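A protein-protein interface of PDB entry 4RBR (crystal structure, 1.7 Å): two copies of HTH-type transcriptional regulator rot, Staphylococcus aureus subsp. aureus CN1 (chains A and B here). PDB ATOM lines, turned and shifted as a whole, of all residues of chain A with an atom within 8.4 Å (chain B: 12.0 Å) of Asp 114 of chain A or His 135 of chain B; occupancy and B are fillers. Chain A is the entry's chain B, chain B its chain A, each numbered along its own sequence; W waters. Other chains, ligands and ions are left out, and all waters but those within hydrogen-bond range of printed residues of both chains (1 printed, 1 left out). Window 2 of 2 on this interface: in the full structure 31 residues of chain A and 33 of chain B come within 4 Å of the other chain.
The backbone NH of His 136 of chain B is in hydrogen-bond range of the side-chain amide oxygen of Asn 110 of chain A (2.9 Å).
A ring nitrogen (NE2) of His 135 of chain B sits at hydrogen-bond distance from the side-chain carboxylate of Asp 114 of chain A, at 2.6 Å.
N of His 135 of chain B is in hydrogen-bond range of OG of Ser 113 of chain A (3.5 Å).
The backbone carbonyl oxygen (O) of Asn 110 of chain A lies within hydrogen-bond range of a ring nitrogen (NE2) of His 135 of chain B.
The backbone carbonyl oxygen of Ala 132 of chain B lies within hydrogen-bond range of a ring nitrogen (ND1) of His 134 of chain B, 2.9 Å away.
Among the printed residues, pairs that only touch across the chains: Ser 113 of chain A with His 134 of chain B (3.1 Å), Ile 116 of chain A with Ile 130 of chain B (3.3 Å), Val 106 of chain A with His 136 of chain B (3.4 Å), Ser 113 of chain A with Val 133 of chain B (3.6 Å), Ala 120 of chain A with Ile 131 of chain B (3.6 Å), Ile 112 of chain A with Ile 12 of chain B (3.7 Å), Leu 109 of chain A with Ile 12 of chain B (3.7 Å), Ile 116 of chain A with Val 133 of chain B (3.97 Å) and Ile 25 of chain A with Leu 15 of chain B (3.99 Å).
Of chain B, only His 135 comes within 4 Å of Asp 114 of chain A.
Of chain A, only Asn 110, Ser 113 and Asp 114 come within 4 Å of His 135 of chain B.
No residue of chain B comes within 4 Å of Phe 111 of chain A.
Of chain B, only Val 133, His 134 and His 135 come within 4 Å of Ser 113 of chain A.
Of chain B, only Ile 130 and Val 133 come within 4 Å of Ile 116 of chain A.
No residue of chain B comes within 4 Å of Ser 118 of chain A.
Of the printed residues of chain A, His 136 of chain B touches Val 106 and Asn 110.
Of the printed residues of chain A, Ile 130 of chain B touches Ile 116.
The nearest residue of chain B that does not touch Asp 114 of chain A is Val 133 of chain B (6.3 Å).
The nearest residue of chain A that does not touch His 135 of chain B is Phe 111 of chain A (5.0 Å).
Printed residues of chain A that touch a printed residue of chain B: Ile 25, Val 106, Leu 109, Asn 110, Ile 112, Ser 113, Asp 114, Ile 116 and Ala 120.
Hydrophobic or aromatic side chains of chain B within 4 Å of the printed part of chain A: Ile 12, Leu 15, Ile 130, Ile 131, Val 133 and His 135.
Among the printed residues, 13 pairs touch across the chains.
Among the printed residues, no Asp or Glu carboxylate lies within 4 Å of a Lys or Arg side-chain nitrogen of the other chain.
No position is printed for both chains.
Of the 13 pairs that touch across the chains among the printed residues, none has its exchanged pair printed and touching as well.
Water W1 lies within hydrogen-bond range of the backbone carbonyl oxygen of Val 133 of chain B (2.7 Å) and the backbone carbonyl oxygen of Ser 113 of chain A (2.8 Å).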
ATOM      1  N   ILE A  25     -22.545  -8.031  -5.176  1.00  0.00           N
ATOM      2  CA  ILE A  25     -22.784  -7.218  -6.357  1.00  0.00           C
ATOM      3  C   ILE A  25     -24.118  -6.496  -6.217  1.00  0.00           C
ATOM      4  O   ILE A  25     -24.196  -5.293  -6.454  1.00  0.00           O
ATOM      5  CB  ILE A  25     -22.775  -8.066  -7.650  1.00  0.00           C
ATOM      6  CG1 ILE A  25     -21.357  -8.576  -7.933  1.00  0.00           C
ATOM      7  CG2 ILE A  25     -23.327  -7.245  -8.818  1.00  0.00           C
ATOM      8  CD1 ILE A  25     -21.302  -9.735  -8.921  1.00  0.00           C
ATOM      9  N   GLU A  28     -23.847  -3.674  -3.790  1.00  0.00           N
ATOM     10  CA  GLU A  28     -23.167  -2.510  -4.354  1.00  0.00           C
ATOM     11  C   GLU A  28     -24.144  -1.643  -5.165  1.00  0.00           C
ATOM     12  O   GLU A  28     -24.159  -0.414  -5.046  1.00  0.00           O
ATOM     13  CB  GLU A  28     -21.977  -2.963  -5.204  1.00  0.00           C
ATOM     14  CG  GLU A  28     -20.883  -3.663  -4.391  1.00  0.00           C
ATOM     15  CD  GLU A  28     -20.011  -4.630  -5.195  1.00  0.00           C
ATOM     16  OE1 GLU A  28     -20.270  -4.832  -6.395  1.00  0.00           O
ATOM     17  OE2 GLU A  28     -19.069  -5.212  -4.604  1.00  0.00           O
ATOM     18  N   VAL A 106     -28.690   3.608 -18.919  1.00  0.00           N
ATOM     19  CA  VAL A 106     -27.397   3.209 -19.449  1.00  0.00           C
ATOM     20  C   VAL A 106     -26.343   3.301 -18.347  1.00  0.00           C
ATOM     21  O   VAL A 106     -25.500   2.413 -18.209  1.00  0.00           O
ATOM     22  CB  VAL A 106     -26.993   4.067 -20.661  1.00  0.00           C
ATOM     23  CG1 VAL A 106     -25.568   3.757 -21.091  1.00  0.00           C
ATOM     24  CG2 VAL A 106     -27.958   3.820 -21.809  1.00  0.00           C
ATOM     25  N   GLU A 107     -26.420   4.358 -17.541  1.00  0.00           N
ATOM     26  CA  GLU A 107     -25.471   4.549 -16.438  1.00  0.00           C
ATOM     27  C   GLU A 107     -25.541   3.415 -15.425  1.00  0.00           C
ATOM     28  O   GLU A 107     -24.523   2.927 -14.939  1.00  0.00           O
ATOM     29  CB  GLU A 107     -25.729   5.877 -15.729  1.00  0.00           C
ATOM     30  CG  GLU A 107     -25.325   7.094 -16.529  1.00  0.00           C
ATOM     31  CD  GLU A 107     -25.989   8.364 -16.026  1.00  0.00           C
ATOM     32  OE1 GLU A 107     -26.500   8.366 -14.878  1.00  0.00           O
ATOM     33  OE2 GLU A 107     -26.013   9.355 -16.789  1.00  0.00           O
ATOM     34  N   LEU A 108     -26.752   3.004 -15.098  1.00  0.00           N
ATOM     35  CA  LEU A 108     -26.934   1.932 -14.129  1.00  0.00           C
ATOM     36  C   LEU A 108     -26.385   0.622 -14.682  1.00  0.00           C
ATOM     37  O   LEU A 108     -25.660  -0.097 -13.990  1.00  0.00           O
ATOM     38  CB  LEU A 108     -28.409   1.787 -13.748  1.00  0.00           C
ATOM     39  CG  LEU A 108     -28.770   0.535 -12.935  1.00  0.00           C
ATOM     40  CD1 LEU A 108     -28.072   0.527 -11.570  1.00  0.00           C
ATOM     41  CD2 LEU A 108     -30.270   0.449 -12.743  1.00  0.00           C
ATOM     42  N   LEU A 109     -26.716   0.313 -15.931  1.00  0.00           N
ATOM     43  CA  LEU A 109     -26.243  -0.927 -16.527  1.00  0.00           C
ATOM     44  C   LEU A 109     -24.725  -0.916 -16.624  1.00  0.00           C
ATOM     45  O   LEU A 109     -24.080  -1.950 -16.437  1.00  0.00           O
ATOM     46  CB  LEU A 109     -26.882  -1.152 -17.903  1.00  0.00           C
ATOM     47  CG  LEU A 109     -28.402  -1.353 -17.880  1.00  0.00           C
ATOM     48  CD1 LEU A 109     -28.971  -1.493 -19.287  1.00  0.00           C
ATOM     49  CD2 LEU A 109     -28.749  -2.570 -17.054  1.00  0.00           C
ATOM     50  N   ASN A 110     -24.144   0.251 -16.903  1.00  0.00           N
ATOM     51  CA  ASN A 110     -22.692   0.347 -16.951  1.00  0.00           C
ATOM     52  C   ASN A 110     -22.079   0.148 -15.579  1.00  0.00           C
ATOM     53  O   ASN A 110     -21.017  -0.456 -15.456  1.00  0.00           O
ATOM     54  CB  ASN A 110     -22.235   1.688 -17.544  1.00  0.00           C
ATOM     55  CG  ASN A 110     -22.365   1.719 -19.052  1.00  0.00           C
ATOM     56  OD1 ASN A 110     -22.560   0.681 -19.676  1.00  0.00           O
ATOM     57  ND2 ASN A 110     -22.241   2.904 -19.645  1.00  0.00           N
ATOM     58  N   PHE A 111     -22.739   0.652 -14.546  1.00  0.00           N
ATOM     59  CA  PHE A 111     -22.221   0.437 -13.205  1.00  0.00           C
ATOM     60  C   PHE A 111     -22.284  -1.051 -12.834  1.00  0.00           C
ATOM     61  O   PHE A 111     -21.365  -1.598 -12.213  1.00  0.00           O
ATOM     62  CB  PHE A 111     -22.989   1.248 -12.163  1.00  0.00           C
ATOM     63  CG  PHE A 111     -22.546   0.951 -10.769  1.00  0.00           C
ATOM     64  CD1 PHE A 111     -21.299   1.383 -10.328  1.00  0.00           C
ATOM     65  CD2 PHE A 111     -23.329   0.179  -9.924  1.00  0.00           C
ATOM     66  CE1 PHE A 111     -20.855   1.075  -9.058  1.00  0.00           C
ATOM     67  CE2 PHE A 111     -22.890  -0.142  -8.662  1.00  0.00           C
ATOM     68  CZ  PHE A 111     -21.653   0.317  -8.220  1.00  0.00           C
ATOM     69  N   ILE A 112     -23.377  -1.702 -13.199  1.00  0.00           N
ATOM     70  CA  ILE A 112     -23.517  -3.114 -12.861  1.00  0.00           C
ATOM     71  C   ILE A 112     -22.425  -3.874 -13.593  1.00  0.00           C
ATOM     72  O   ILE A 112     -21.780  -4.747 -13.014  1.00  0.00           O
ATOM     73  CB  ILE A 112     -24.914  -3.660 -13.209  1.00  0.00           C
ATOM     74  CG1 ILE A 112     -25.986  -2.901 -12.435  1.00  0.00           C
ATOM     75  CG2 ILE A 112     -25.006  -5.161 -12.888  1.00  0.00           C
ATOM     76  CD1 ILE A 112     -27.394  -3.294 -12.773  1.00  0.00           C
ATOM     77  N   SER A 113     -22.194  -3.517 -14.852  1.00  0.00           N
ATOM     78  CA  SER A 113     -21.102  -4.094 -15.615  1.00  0.00           C
ATOM     79  C   SER A 113     -19.769  -3.946 -14.874  1.00  0.00           C
ATOM     80  O   SER A 113     -18.982  -4.897 -14.807  1.00  0.00           O
ATOM     81  CB  SER A 113     -21.016  -3.439 -16.990  1.00  0.00           C
ATOM     82  OG  SER A 113     -19.955  -3.982 -17.748  1.00  0.00           O
ATOM     83  N   ASP A 114     -19.519  -2.748 -14.337  1.00  0.00           N
ATOM     84  CA  ASP A 114     -18.297  -2.482 -13.562  1.00  0.00           C
ATOM     85  C   ASP A 114     -18.179  -3.408 -12.370  1.00  0.00           C
ATOM     86  O   ASP A 114     -17.121  -3.963 -12.104  1.00  0.00           O
ATOM     87  CB  ASP A 114     -18.255  -1.036 -13.040  1.00  0.00           C
ATOM     88  CG  ASP A 114     -18.047  -0.014 -14.128  1.00  0.00           C
ATOM     89  OD1 ASP A 114     -17.681  -0.398 -15.261  1.00  0.00           O
ATOM     90  OD2 ASP A 114     -18.233   1.192 -13.830  1.00  0.00           O
ATOM     91  N   ALA A 115     -19.264  -3.540 -11.620  1.00  0.00           N
ATOM     92  CA  ALA A 115     -19.246  -4.329 -10.407  1.00  0.00           C
ATOM     93  C   ALA A 115     -19.015  -5.790 -10.756  1.00  0.00           C
ATOM     94  O   ALA A 115     -18.336  -6.497 -10.032  1.00  0.00           O
ATOM     95  CB  ALA A 115     -20.548  -4.162  -9.631  1.00  0.00           C
ATOM     96  N   ILE A 116     -19.583  -6.230 -11.877  1.00  0.00           N
ATOM     97  CA  ILE A 116     -19.383  -7.611 -12.308  1.00  0.00           C
ATOM     98  C   ILE A 116     -17.935  -7.811 -12.715  1.00  0.00           C
ATOM     99  O   ILE A 116     -17.314  -8.813 -12.370  1.00  0.00           O
ATOM    100  CB  ILE A 116     -20.326  -7.978 -13.481  1.00  0.00           C
ATOM    101  CG1 ILE A 116     -21.769  -8.037 -12.993  1.00  0.00           C
ATOM    102  CG2 ILE A 116     -19.914  -9.311 -14.135  1.00  0.00           C
ATOM    103  CD1 ILE A 116     -22.776  -8.257 -14.135  1.00  0.00           C
ATOM    104  N   ALA A 117     -17.393  -6.826 -13.427  1.00  0.00           N
ATOM    105  CA  ALA A 117     -16.036  -6.924 -13.950  1.00  0.00           C
ATOM    106  C   ALA A 117     -15.020  -6.972 -12.813  1.00  0.00           C
ATOM    107  O   ALA A 117     -14.005  -7.667 -12.902  1.00  0.00           O
ATOM    108  CB  ALA A 117     -15.736  -5.763 -14.881  1.00  0.00           C
ATOM    109  N   SER A 118     -15.298  -6.240 -11.739  1.00  0.00           N
ATOM    110  CA  SER A 118     -14.364  -6.217 -10.617  1.00  0.00           C
ATOM    111  C   SER A 118     -14.369  -7.547  -9.852  1.00  0.00           C
ATOM    112  O   SER A 118     -13.455  -7.819  -9.085  1.00  0.00           O
ATOM    113  CB  SER A 118     -14.676  -5.056  -9.656  1.00  0.00           C
ATOM    114  OG  SER A 118     -15.868  -5.283  -8.937  1.00  0.00           O
ATOM    115  N   ARG A 119     -15.393  -8.370 -10.086  1.00  0.00           N
ATOM    116  CA  ARG A 119     -15.560  -9.635  -9.376  1.00  0.00           C
ATOM    117  C   ARG A 119     -15.347 -10.855 -10.270  1.00  0.00           C
ATOM    118  O   ARG A 119     -15.349 -11.974  -9.784  1.00  0.00           O
ATOM    119  CB  ARG A 119     -16.975  -9.699  -8.759  1.00  0.00           C
ATOM    120  CG  ARG A 119     -17.055 -10.392  -7.418  1.00  0.00           C
ATOM    121  CD  ARG A 119     -16.227  -9.644  -6.392  1.00  0.00           C
ATOM    122  NE  ARG A 119     -16.619  -9.971  -5.029  1.00  0.00           N
ATOM    123  CZ  ARG A 119     -17.447  -9.237  -4.298  1.00  0.00           C
ATOM    124  NH1 ARG A 119     -17.739  -9.620  -3.064  1.00  0.00           N
ATOM    125  NH2 ARG A 119     -17.966  -8.111  -4.793  1.00  0.00           N
ATOM    126  N   ALA A 120     -15.175 -10.634 -11.571  1.00  0.00           N
ATOM    127  CA  ALA A 120     -15.305 -11.713 -12.551  1.00  0.00           C
ATOM    128  C   ALA A 120     -14.281 -12.822 -12.350  1.00  0.00           C
ATOM    129  O   ALA A 120     -14.625 -14.005 -12.413  1.00  0.00           O
ATOM    130  CB  ALA A 120     -15.203 -11.161 -13.969  1.00  0.00           C
ATOM    131  N   ASN B   6     -32.251  -8.018 -24.386  1.00  0.00           N
ATOM    132  CA  ASN B   6     -30.997  -7.308 -24.147  1.00  0.00           C
ATOM    133  C   ASN B   6     -29.889  -8.263 -23.695  1.00  0.00           C
ATOM    134  O   ASN B   6     -30.047  -8.988 -22.728  1.00  0.00           O
ATOM    135  CB  ASN B   6     -31.216  -6.218 -23.102  1.00  0.00           C
ATOM    136  CG  ASN B   6     -30.013  -5.315 -22.918  1.00  0.00           C
ATOM    137  OD1 ASN B   6     -28.872  -5.761 -22.933  1.00  0.00           O
ATOM    138  ND2 ASN B   6     -30.273  -4.024 -22.742  1.00  0.00           N
ATOM    139  N   ASP B   7     -28.779  -8.256 -24.427  1.00  0.00           N
ATOM    140  CA  ASP B   7     -27.562  -9.011 -24.119  1.00  0.00           C
ATOM    141  C   ASP B   7     -27.033  -8.672 -22.714  1.00  0.00           C
ATOM    142  O   ASP B   7     -26.710  -9.559 -21.914  1.00  0.00           O
ATOM    143  CB  ASP B   7     -26.510  -8.705 -25.203  1.00  0.00           C
ATOM    144  CG  ASP B   7     -25.231  -9.509 -25.050  1.00  0.00           C
ATOM    145  OD1 ASP B   7     -25.234 -10.548 -24.352  1.00  0.00           O
ATOM    146  OD2 ASP B   7     -24.212  -9.101 -25.657  1.00  0.00           O
ATOM    147  N   THR B   8     -26.950  -7.379 -22.423  1.00  0.00           N
ATOM    148  CA  THR B   8     -26.520  -6.913 -21.113  1.00  0.00           C
ATOM    149  C   THR B   8     -27.535  -7.248 -20.041  1.00  0.00           C
ATOM    150  O   THR B   8     -27.186  -7.766 -18.989  1.00  0.00           O
ATOM    151  CB  THR B   8     -26.300  -5.393 -21.111  1.00  0.00           C
ATOM    152  OG1 THR B   8     -25.401  -5.046 -22.172  1.00  0.00           O
ATOM    153  CG2 THR B   8     -25.727  -4.939 -19.776  1.00  0.00           C
ATOM    154  N   VAL B   9     -28.799  -6.938 -20.298  1.00  0.00           N
ATOM    155  CA  VAL B   9     -29.807  -7.145 -19.273  1.00  0.00           C
ATOM    156  C   VAL B   9     -30.001  -8.636 -18.982  1.00  0.00           C
ATOM    157  O   VAL B   9     -30.149  -9.023 -17.826  1.00  0.00           O
ATOM    158  CB  VAL B   9     -31.147  -6.500 -19.668  1.00  0.00           C
ATOM    159  CG1 VAL B   9     -32.234  -6.936 -18.738  1.00  0.00           C
ATOM    160  CG2 VAL B   9     -31.010  -4.984 -19.658  1.00  0.00           C
ATOM    161  N   GLY B  11     -27.747 -10.965 -19.233  1.00  0.00           N
ATOM    162  CA  GLY B  11     -26.564 -11.381 -18.509  1.00  0.00           C
ATOM    163  C   GLY B  11     -26.595 -10.998 -17.042  1.00  0.00           C
ATOM    164  O   GLY B  11     -26.225 -11.794 -16.177  1.00  0.00           O
ATOM    165  N   ILE B  12     -27.032  -9.776 -16.749  1.00  0.00           N
ATOM    166  CA  ILE B  12     -27.146  -9.352 -15.354  1.00  0.00           C
ATOM    167  C   ILE B  12     -28.193 -10.203 -14.634  1.00  0.00           C
ATOM    168  O   ILE B  12     -27.998 -10.607 -13.485  1.00  0.00           O
ATOM    169  CB  ILE B  12     -27.494  -7.842 -15.245  1.00  0.00           C
ATOM    170  CG1 ILE B  12     -26.338  -6.995 -15.779  1.00  0.00           C
ATOM    171  CG2 ILE B  12     -27.762  -7.453 -13.794  1.00  0.00           C
ATOM    172  CD1 ILE B  12     -26.750  -5.582 -16.212  1.00  0.00           C
ATOM    173  N   LEU B  15     -27.384 -13.410 -12.834  1.00  0.00           N
ATOM    174  CA  LEU B  15     -26.881 -13.389 -11.464  1.00  0.00           C
ATOM    175  C   LEU B  15     -27.854 -14.130 -10.561  1.00  0.00           C
ATOM    176  O   LEU B  15     -27.453 -14.930  -9.714  1.00  0.00           O
ATOM    177  CB  LEU B  15     -26.679 -11.947 -10.966  1.00  0.00           C
ATOM    178  CG  LEU B  15     -25.452 -11.194 -11.471  1.00  0.00           C
ATOM    179  CD1 LEU B  15     -25.592  -9.702 -11.156  1.00  0.00           C
ATOM    180  CD2 LEU B  15     -24.164 -11.730 -10.866  1.00  0.00           C
ATOM    181  N   ALA B 129     -22.648 -15.858 -19.068  1.00  0.00           N
ATOM    182  CA  ALA B 129     -23.557 -14.776 -19.445  1.00  0.00           C
ATOM    183  C   ALA B 129     -23.316 -13.558 -18.553  1.00  0.00           C
ATOM    184  O   ALA B 129     -23.319 -12.411 -19.012  1.00  0.00           O
ATOM    185  CB  ALA B 129     -25.004 -15.236 -19.360  1.00  0.00           C
ATOM    186  N   ILE B 130     -23.090 -13.818 -17.272  1.00  0.00           N
ATOM    187  CA  ILE B 130     -22.817 -12.746 -16.318  1.00  0.00           C
ATOM    188  C   ILE B 130     -21.552 -11.972 -16.676  1.00  0.00           C
ATOM    189  O   ILE B 130     -21.549 -10.745 -16.681  1.00  0.00           O
ATOM    190  CB  ILE B 130     -22.677 -13.312 -14.893  1.00  0.00           C
ATOM    191  CG1 ILE B 130     -24.017 -13.856 -14.392  1.00  0.00           C
ATOM    192  CG2 ILE B 130     -22.097 -12.248 -13.936  1.00  0.00           C
ATOM    193  CD1 ILE B 130     -23.866 -14.809 -13.218  1.00  0.00           C
ATOM    194  N   ILE B 131     -20.473 -12.690 -16.976  1.00  0.00           N
ATOM    195  CA  ILE B 131     -19.157 -12.082 -17.145  1.00  0.00           C
ATOM    196  C   ILE B 131     -19.055 -11.403 -18.512  1.00  0.00           C
ATOM    197  O   ILE B 131     -18.304 -10.445 -18.693  1.00  0.00           O
ATOM    198  CB  ILE B 131     -18.038 -13.149 -16.956  1.00  0.00           C
ATOM    199  CG1 ILE B 131     -17.963 -13.530 -15.475  1.00  0.00           C
ATOM    200  CG2 ILE B 131     -16.663 -12.658 -17.466  1.00  0.00           C
ATOM    201  CD1 ILE B 131     -16.878 -14.532 -15.132  1.00  0.00           C
ATOM    202  N   ALA B 132     -19.889 -11.861 -19.440  1.00  0.00           N
ATOM    203  CA  ALA B 132     -19.987 -11.261 -20.764  1.00  0.00           C
ATOM    204  C   ALA B 132     -20.607  -9.860 -20.749  1.00  0.00           C
ATOM    205  O   ALA B 132     -20.490  -9.128 -21.736  1.00  0.00           O
ATOM    206  CB  ALA B 132     -20.790 -12.166 -21.683  1.00  0.00           C
ATOM    207  N   VAL B 133     -21.274  -9.506 -19.646  1.00  0.00           N
ATOM    208  CA  VAL B 133     -21.864  -8.173 -19.475  1.00  0.00           C
ATOM    209  C   VAL B 133     -20.781  -7.111 -19.638  1.00  0.00           C
ATOM    210  O   VAL B 133     -19.669  -7.251 -19.116  1.00  0.00           O
ATOM    211  CB  VAL B 133     -22.554  -8.022 -18.089  1.00  0.00           C
ATOM    212  CG1 VAL B 133     -23.019  -6.569 -17.842  1.00  0.00           C
ATOM    213  CG2 VAL B 133     -23.738  -8.982 -17.968  1.00  0.00           C
ATOM    214  N   HIS B 134     -21.083  -6.056 -20.386  1.00  0.00           N
ATOM    215  CA  HIS B 134     -20.069  -5.034 -20.619  1.00  0.00           C
ATOM    216  C   HIS B 134     -20.667  -3.637 -20.795  1.00  0.00           C
ATOM    217  O   HIS B 134     -21.885  -3.452 -20.758  1.00  0.00           O
ATOM    218  CB  HIS B 134     -19.217  -5.412 -21.832  1.00  0.00           C
ATOM    219  CG  HIS B 134     -20.007  -5.576 -23.091  1.00  0.00           C
ATOM    220  ND1 HIS B 134     -20.608  -6.766 -23.442  1.00  0.00           N
ATOM    221  CD2 HIS B 134     -20.306  -4.696 -24.076  1.00  0.00           C
ATOM    222  CE1 HIS B 134     -21.238  -6.613 -24.593  1.00  0.00           C
ATOM    223  NE2 HIS B 134     -21.070  -5.366 -24.998  1.00  0.00           N
ATOM    224  N   HIS B 135     -19.796  -2.649 -20.957  1.00  0.00           N
ATOM    225  CA  HIS B 135     -20.226  -1.263 -21.109  1.00  0.00           C
ATOM    226  C   HIS B 135     -20.872  -0.967 -22.448  1.00  0.00           C
ATOM    227  O   HIS B 135     -20.522  -1.569 -23.463  1.00  0.00           O
ATOM    228  CB  HIS B 135     -19.039  -0.318 -20.939  1.00  0.00           C
ATOM    229  CG  HIS B 135     -18.892   0.236 -19.559  1.00  0.00           C
ATOM    230  ND1 HIS B 135     -18.902   1.589 -19.300  1.00  0.00           N
ATOM    231  CD2 HIS B 135     -18.719  -0.376 -18.363  1.00  0.00           C
ATOM    232  CE1 HIS B 135     -18.741   1.786 -18.002  1.00  0.00           C
ATOM    233  NE2 HIS B 135     -18.626   0.609 -17.413  1.00  0.00           N
ATOM    234  N   HIS B 136     -21.819  -0.032 -22.426  1.00  0.00           N
ATOM    235  CA  HIS B 136     -22.268   0.677 -23.620  1.00  0.00           C
ATOM    236  C   HIS B 136     -23.158   1.851 -23.224  1.00  0.00           C
ATOM    237  O   HIS B 136     -22.681   2.834 -22.648  1.00  0.00           O
ATOM    238  CB  HIS B 136     -23.011  -0.239 -24.588  1.00  0.00           C
ATOM    239  CG  HIS B 136     -22.712   0.058 -26.025  1.00  0.00           C
ATOM    240  ND1 HIS B 136     -21.537   0.661 -26.426  1.00  0.00           N
ATOM    241  CD2 HIS B 136     -23.432  -0.146 -27.154  1.00  0.00           C
ATOM    242  CE1 HIS B 136     -21.543   0.807 -27.737  1.00  0.00           C
ATOM    243  NE2 HIS B 136     -22.682   0.325 -28.204  1.00  0.00           N
HETATM  244  O   HOH W   1     -18.269  -6.753 -16.840  1.00  0.00           O
